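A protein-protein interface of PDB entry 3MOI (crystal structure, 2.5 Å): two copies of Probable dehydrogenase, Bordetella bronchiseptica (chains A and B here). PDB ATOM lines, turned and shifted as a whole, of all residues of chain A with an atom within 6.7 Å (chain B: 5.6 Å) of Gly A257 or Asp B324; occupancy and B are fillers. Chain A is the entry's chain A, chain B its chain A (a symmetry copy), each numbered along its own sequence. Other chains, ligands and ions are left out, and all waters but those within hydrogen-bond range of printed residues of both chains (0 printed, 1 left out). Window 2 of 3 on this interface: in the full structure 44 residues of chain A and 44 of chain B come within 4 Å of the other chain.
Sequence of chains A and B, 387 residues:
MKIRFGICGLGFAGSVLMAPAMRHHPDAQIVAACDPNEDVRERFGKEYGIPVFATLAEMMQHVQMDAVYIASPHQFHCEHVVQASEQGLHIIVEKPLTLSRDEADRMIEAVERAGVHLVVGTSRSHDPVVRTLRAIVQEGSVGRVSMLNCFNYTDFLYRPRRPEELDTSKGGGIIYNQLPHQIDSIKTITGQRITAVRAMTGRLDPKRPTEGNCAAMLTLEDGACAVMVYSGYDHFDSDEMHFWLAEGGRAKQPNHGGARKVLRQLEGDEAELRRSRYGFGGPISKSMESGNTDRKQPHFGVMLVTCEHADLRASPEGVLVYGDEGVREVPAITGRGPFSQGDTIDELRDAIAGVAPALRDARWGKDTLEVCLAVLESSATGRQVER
No position is printed for both chains. Of the 10 pairs that touch across the chains among the printed residues, none has its exchanged pair printed and touching as well.
The side-chain carboxylate (OD2) of Asp A234 lies close to the backbone carbonyl oxygen (O) of His A256, at 2.7 Å. The guanidinium group (NH2) of Arg A260 is in hydrogen-bond range of a ring nitrogen (NE2) of His A235, 3.3 Å away. The backbone carbonyl oxygen (O) of Tyr A233 is in hydrogen-bond range of the guanidinium group (NH2) of Arg A260 (2.6 Å). OD1 of Asp A234 is in hydrogen-bond range of N of Arg A260, at 3.3 Å.
Printed residues of chain A that touch a printed residue of chain B: His A235, His A256, Gly A257 and Arg A260. Among the printed residues, Asp or Glu carboxylates within 4 Å of a Lys or Arg side-chain nitrogen of the other chain: Arg A260 with Asp B324.
Among the printed residues, merely in contact across the chains: His A235 with Ala B310, His A235 with Tyr B322, His A235 with Gly B323, His A256 with Tyr B322, His A235 with Glu B308, Gly A257 with Gly B326 and Gly A257 with Asp B324.
Printed residues of chain B within 4 Å of Gly A257: Asp B324 (3.99 Å) and Gly B326 (3.9 Å). Of the printed residues of chain A, Asp B324 touches His A235 (2.8 Å), Gly A257 (3.99 Å) and Arg A260 (3.0 Å). Of the printed residues of chain A, Glu B308 touches His A235. Of the printed residues of chain A, Tyr B322 touches His A235 and His A256. Of the printed residues of chain B, Arg A260 touches Asp B324 (3.0 Å). Printed residues of chain A within 4 Å of Gly B326: Gly A257. Printed residues of chain A within 4 Å of Ala B310: His A235. Asp A234 touches none of the printed residues of chain B. Ala A259 touches none of the printed residues of chain B. The nearest printed residue of chain A that does not touch Asp B324 is His A256 (5.0 Å).
A ring nitrogen (NE2) of His A235 lies within hydrogen-bond range of the side-chain carboxylate (OD1) of Asp B324, 2.8 Å away. A ring nitrogen (NE2) of His A235 is in hydrogen-bond range of the backbone carbonyl oxygen (O) of His B309 (3.5 Å). The side-chain carboxylate (OD1) of Asp B324 lies within salt-bridge range of the guanidinium group (NH2) of Arg A260 (3.0 Å).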
ATOM      1  N   TYR A 158      14.982  14.122   9.150  1.00  0.00           N
ATOM      2  CA  TYR A 158      14.373  12.814   9.064  1.00  0.00           C
ATOM      3  C   TYR A 158      13.220  12.728   8.053  1.00  0.00           C
ATOM      4  O   TYR A 158      12.477  11.790   8.086  1.00  0.00           O
ATOM      5  CB  TYR A 158      13.967  12.333  10.457  1.00  0.00           C
ATOM      6  CG  TYR A 158      15.208  12.136  11.316  1.00  0.00           C
ATOM      7  CD1 TYR A 158      15.910  10.933  11.314  1.00  0.00           C
ATOM      8  CD2 TYR A 158      15.731  13.180  12.055  1.00  0.00           C
ATOM      9  CE1 TYR A 158      17.079  10.767  12.081  1.00  0.00           C
ATOM     10  CE2 TYR A 158      16.884  13.014  12.802  1.00  0.00           C
ATOM     11  CZ  TYR A 158      17.544  11.809  12.808  1.00  0.00           C
ATOM     12  OH  TYR A 158      18.671  11.695  13.570  1.00  0.00           O
ATOM     13  N   TYR A 233      16.295  17.651  14.071  1.00  0.00           N
ATOM     14  CA  TYR A 233      16.394  16.243  14.482  1.00  0.00           C
ATOM     15  C   TYR A 233      15.040  15.634  14.856  1.00  0.00           C
ATOM     16  O   TYR A 233      14.978  14.502  15.342  1.00  0.00           O
ATOM     17  CB  TYR A 233      17.415  16.120  15.623  1.00  0.00           C
ATOM     18  CG  TYR A 233      18.825  16.558  15.206  1.00  0.00           C
ATOM     19  CD1 TYR A 233      19.574  15.818  14.288  1.00  0.00           C
ATOM     20  CD2 TYR A 233      19.402  17.718  15.722  1.00  0.00           C
ATOM     21  CE1 TYR A 233      20.858  16.222  13.892  1.00  0.00           C
ATOM     22  CE2 TYR A 233      20.694  18.145  15.311  1.00  0.00           C
ATOM     23  CZ  TYR A 233      21.402  17.390  14.398  1.00  0.00           C
ATOM     24  OH  TYR A 233      22.649  17.783  14.014  1.00  0.00           O
ATOM     25  N   ASP A 234      13.953  16.373  14.618  1.00  0.00           N
ATOM     26  CA  ASP A 234      12.606  15.892  14.895  1.00  0.00           C
ATOM     27  C   ASP A 234      12.354  15.693  16.389  1.00  0.00           C
ATOM     28  O   ASP A 234      11.633  14.742  16.811  1.00  0.00           O
ATOM     29  CB  ASP A 234      12.324  14.576  14.165  1.00  0.00           C
ATOM     30  CG  ASP A 234      10.831  14.251  14.113  1.00  0.00           C
ATOM     31  OD1 ASP A 234      10.485  13.183  13.543  1.00  0.00           O
ATOM     32  OD2 ASP A 234      10.013  15.062  14.656  1.00  0.00           O
ATOM     33  N   HIS A 235      12.937  16.587  17.194  1.00  0.00           N
ATOM     34  CA  HIS A 235      12.735  16.545  18.631  1.00  0.00           C
ATOM     35  C   HIS A 235      11.781  17.675  18.940  1.00  0.00           C
ATOM     36  O   HIS A 235      10.615  17.560  18.642  1.00  0.00           O
ATOM     37  CB  HIS A 235      14.050  16.672  19.343  1.00  0.00           C
ATOM     38  CG  HIS A 235      14.913  15.464  19.215  1.00  0.00           C
ATOM     39  ND1 HIS A 235      16.292  15.527  19.289  1.00  0.00           N
ATOM     40  CD2 HIS A 235      14.599  14.161  19.016  1.00  0.00           C
ATOM     41  CE1 HIS A 235      16.788  14.305  19.157  1.00  0.00           C
ATOM     42  NE2 HIS A 235      15.784  13.459  18.988  1.00  0.00           N
ATOM     43  N   ASN A 255       3.232  15.612  15.966  1.00  0.00           N
ATOM     44  CA  ASN A 255       3.711  14.289  15.537  1.00  0.00           C
ATOM     45  C   ASN A 255       5.241  14.112  15.799  1.00  0.00           C
ATOM     46  O   ASN A 255       6.034  13.795  14.916  1.00  0.00           O
ATOM     47  CB  ASN A 255       3.349  14.073  14.047  1.00  0.00           C
ATOM     48  CG  ASN A 255       3.410  12.586  13.610  1.00  0.00           C
ATOM     49  OD1 ASN A 255       2.891  11.678  14.268  1.00  0.00           O
ATOM     50  ND2 ASN A 255       4.052  12.354  12.481  1.00  0.00           N
ATOM     51  N   HIS A 256       5.647  14.276  17.042  1.00  0.00           N
ATOM     52  CA  HIS A 256       7.051  14.341  17.361  1.00  0.00           C
ATOM     53  C   HIS A 256       7.887  13.121  16.929  1.00  0.00           C
ATOM     54  O   HIS A 256       8.906  13.225  16.274  1.00  0.00           O
ATOM     55  CB  HIS A 256       7.184  14.648  18.834  1.00  0.00           C
ATOM     56  CG  HIS A 256       6.485  15.910  19.244  1.00  0.00           C
ATOM     57  ND1 HIS A 256       7.137  17.111  19.377  1.00  0.00           N
ATOM     58  CD2 HIS A 256       5.194  16.153  19.562  1.00  0.00           C
ATOM     59  CE1 HIS A 256       6.284  18.041  19.763  1.00  0.00           C
ATOM     60  NE2 HIS A 256       5.099  17.483  19.892  1.00  0.00           N
ATOM     61  N   GLY A 257       7.469  11.935  17.265  1.00  0.00           N
ATOM     62  CA  GLY A 257       8.102  10.767  16.612  1.00  0.00           C
ATOM     63  C   GLY A 257       8.202  10.941  15.083  1.00  0.00           C
ATOM     64  O   GLY A 257       9.236  10.672  14.456  1.00  0.00           O
ATOM     65  N   GLY A 258       7.106  11.428  14.518  1.00  0.00           N
ATOM     66  CA  GLY A 258       6.856  11.508  13.076  1.00  0.00           C
ATOM     67  C   GLY A 258       7.802  10.930  12.050  1.00  0.00           C
ATOM     68  O   GLY A 258       7.685   9.769  11.678  1.00  0.00           O
ATOM     69  N   ALA A 259       8.726  11.762  11.586  1.00  0.00           N
ATOM     70  CA  ALA A 259       9.492  11.451  10.406  1.00  0.00           C
ATOM     71  C   ALA A 259      10.498  10.365  10.677  1.00  0.00           C
ATOM     72  O   ALA A 259      10.839   9.609   9.781  1.00  0.00           O
ATOM     73  CB  ALA A 259      10.192  12.744   9.865  1.00  0.00           C
ATOM     74  N   ARG A 260      10.990  10.311  11.905  1.00  0.00           N
ATOM     75  CA  ARG A 260      11.900   9.258  12.337  1.00  0.00           C
ATOM     76  C   ARG A 260      11.188   7.871  12.452  1.00  0.00           C
ATOM     77  O   ARG A 260      11.778   6.846  12.105  1.00  0.00           O
ATOM     78  CB  ARG A 260      12.565   9.645  13.670  1.00  0.00           C
ATOM     79  CG  ARG A 260      13.590   8.611  14.155  1.00  0.00           C
ATOM     80  CD  ARG A 260      14.048   8.807  15.621  1.00  0.00           C
ATOM     81  NE  ARG A 260      15.036   9.891  15.728  1.00  0.00           N
ATOM     82  CZ  ARG A 260      14.748  11.180  15.910  1.00  0.00           C
ATOM     83  NH1 ARG A 260      13.476  11.568  16.050  1.00  0.00           N
ATOM     84  NH2 ARG A 260      15.745  12.076  15.991  1.00  0.00           N
ATOM     85  N   LYS A 261       9.943   7.849  12.936  1.00  0.00           N
ATOM     86  CA  LYS A 261       9.123   6.624  12.950  1.00  0.00           C
ATOM     87  C   LYS A 261       8.975   6.103  11.529  1.00  0.00           C
ATOM     88  O   LYS A 261       9.366   4.984  11.227  1.00  0.00           O
ATOM     89  CB  LYS A 261       7.726   6.909  13.542  1.00  0.00           C
ATOM     90  CG  LYS A 261       6.934   5.685  14.080  1.00  0.00           C
ATOM     91  CD  LYS A 261       5.486   6.054  14.590  1.00  0.00           C
ATOM     92  CE  LYS A 261       5.390   7.511  15.246  1.00  0.00           C
ATOM     93  NZ  LYS A 261       6.218   7.782  16.522  1.00  0.00           N
ATOM     94  N   VAL A 262       8.446   6.941  10.651  1.00  0.00           N
ATOM     95  CA  VAL A 262       8.266   6.553   9.254  1.00  0.00           C
ATOM     96  C   VAL A 262       9.538   5.894   8.698  1.00  0.00           C
ATOM     97  O   VAL A 262       9.456   4.884   8.016  1.00  0.00           O
ATOM     98  CB  VAL A 262       7.790   7.729   8.359  1.00  0.00           C
ATOM     99  CG1 VAL A 262       7.902   7.358   6.914  1.00  0.00           C
ATOM    100  CG2 VAL A 262       6.353   8.150   8.695  1.00  0.00           C
ATOM    101  N   ARG A 264      12.163   4.390  10.361  1.00  0.00           N
ATOM    102  CA  ARG A 264      12.644   3.208  11.088  1.00  0.00           C
ATOM    103  C   ARG A 264      11.882   1.933  10.632  1.00  0.00           C
ATOM    104  O   ARG A 264      12.473   0.851  10.434  1.00  0.00           O
ATOM    105  CB  ARG A 264      12.496   3.459  12.598  1.00  0.00           C
ATOM    106  CG  ARG A 264      12.968   2.322  13.508  1.00  0.00           C
ATOM    107  CD  ARG A 264      12.906   2.684  15.038  1.00  0.00           C
ATOM    108  NE  ARG A 264      11.647   3.325  15.483  1.00  0.00           N
ATOM    109  CZ  ARG A 264      10.460   2.716  15.644  1.00  0.00           C
ATOM    110  NH1 ARG A 264      10.287   1.421  15.390  1.00  0.00           N
ATOM    111  NH2 ARG A 264       9.415   3.422  16.058  1.00  0.00           N
ATOM    112  N   GLU B 308      22.091  15.289  21.681  1.00  0.00           N
ATOM    113  CA  GLU B 308      22.132  14.252  20.653  1.00  0.00           C
ATOM    114  C   GLU B 308      20.793  13.482  20.561  1.00  0.00           C
ATOM    115  O   GLU B 308      20.293  13.257  19.491  1.00  0.00           O
ATOM    116  CB  GLU B 308      23.242  13.224  20.947  1.00  0.00           C
ATOM    117  CG  GLU B 308      24.670  13.624  20.580  1.00  0.00           C
ATOM    118  CD  GLU B 308      25.790  12.786  21.310  1.00  0.00           C
ATOM    119  OE1 GLU B 308      25.628  12.302  22.486  1.00  0.00           O
ATOM    120  OE2 GLU B 308      26.860  12.656  20.659  1.00  0.00           O
ATOM    121  N   HIS B 309      20.222  13.077  21.685  1.00  0.00           N
ATOM    122  CA  HIS B 309      19.047  12.199  21.606  1.00  0.00           C
ATOM    123  C   HIS B 309      17.746  12.879  22.048  1.00  0.00           C
ATOM    124  O   HIS B 309      16.708  12.232  22.119  1.00  0.00           O
ATOM    125  CB  HIS B 309      19.315  10.847  22.334  1.00  0.00           C
ATOM    126  CG  HIS B 309      20.456  10.061  21.733  1.00  0.00           C
ATOM    127  ND1 HIS B 309      21.539   9.625  22.469  1.00  0.00           N
ATOM    128  CD2 HIS B 309      20.705   9.698  20.454  1.00  0.00           C
ATOM    129  CE1 HIS B 309      22.395   9.011  21.670  1.00  0.00           C
ATOM    130  NE2 HIS B 309      21.908   9.040  20.444  1.00  0.00           N
ATOM    131  N   ALA B 310      17.765  14.197  22.219  1.00  0.00           N
ATOM    132  CA  ALA B 310      16.577  14.894  22.671  1.00  0.00           C
ATOM    133  C   ALA B 310      16.764  16.401  22.709  1.00  0.00           C
ATOM    134  O   ALA B 310      17.896  16.858  22.802  1.00  0.00           O
ATOM    135  CB  ALA B 310      16.210  14.409  24.084  1.00  0.00           C
ATOM    136  N   TYR B 322      11.756  15.982  24.598  1.00  0.00           N
ATOM    137  CA  TYR B 322      11.327  15.660  23.227  1.00  0.00           C
ATOM    138  C   TYR B 322      12.280  14.673  22.631  1.00  0.00           C
ATOM    139  O   TYR B 322      13.314  15.052  22.117  1.00  0.00           O
ATOM    140  CB  TYR B 322      11.273  16.916  22.378  1.00  0.00           C
ATOM    141  CG  TYR B 322      10.238  17.878  22.880  1.00  0.00           C
ATOM    142  CD1 TYR B 322       8.915  17.872  22.392  1.00  0.00           C
ATOM    143  CD2 TYR B 322      10.547  18.767  23.888  1.00  0.00           C
ATOM    144  CE1 TYR B 322       7.955  18.793  22.902  1.00  0.00           C
ATOM    145  CE2 TYR B 322       9.614  19.669  24.373  1.00  0.00           C
ATOM    146  CZ  TYR B 322       8.344  19.686  23.898  1.00  0.00           C
ATOM    147  OH  TYR B 322       7.502  20.619  24.441  1.00  0.00           O
ATOM    148  N   GLY B 323      11.923  13.387  22.676  1.00  0.00           N
ATOM    149  CA  GLY B 323      12.883  12.347  22.333  1.00  0.00           C
ATOM    150  C   GLY B 323      12.725  11.860  20.928  1.00  0.00           C
ATOM    151  O   GLY B 323      11.879  12.340  20.188  1.00  0.00           O
ATOM    152  N   ASP B 324      13.567  10.890  20.578  1.00  0.00           N
ATOM    153  CA  ASP B 324      13.460  10.135  19.331  1.00  0.00           C
ATOM    154  C   ASP B 324      12.057   9.514  19.192  1.00  0.00           C
ATOM    155  O   ASP B 324      11.523   9.359  18.104  1.00  0.00           O
ATOM    156  CB  ASP B 324      14.528   9.009  19.310  1.00  0.00           C
ATOM    157  CG  ASP B 324      15.959   9.518  18.984  1.00  0.00           C
ATOM    158  OD1 ASP B 324      16.123  10.718  18.680  1.00  0.00           O
ATOM    159  OD2 ASP B 324      16.928   8.713  19.047  1.00  0.00           O
ATOM    160  N   GLU B 325      11.482   9.171  20.331  1.00  0.00           N
ATOM    161  CA  GLU B 325      10.284   8.330  20.389  1.00  0.00           C
ATOM    162  C   GLU B 325       9.047   9.198  20.478  1.00  0.00           C
ATOM    163  O   GLU B 325       7.940   8.667  20.412  1.00  0.00           O
ATOM    164  CB  GLU B 325      10.349   7.455  21.660  1.00  0.00           C
ATOM    165  CG  GLU B 325       9.756   6.085  21.549  1.00  0.00           C
ATOM    166  CD  GLU B 325      10.586   5.173  20.652  1.00  0.00           C
ATOM    167  OE1 GLU B 325      10.540   3.914  20.866  1.00  0.00           O
ATOM    168  OE2 GLU B 325      11.271   5.746  19.751  1.00  0.00           O
ATOM    169  N   GLY B 326       9.246  10.511  20.665  1.00  0.00           N
ATOM    170  CA  GLY B 326       8.165  11.424  21.023  1.00  0.00           C
ATOM    171  C   GLY B 326       8.427  12.026  22.398  1.00  0.00           C
ATOM    172  O   GLY B 326       9.449  11.772  22.997  1.00  0.00           O
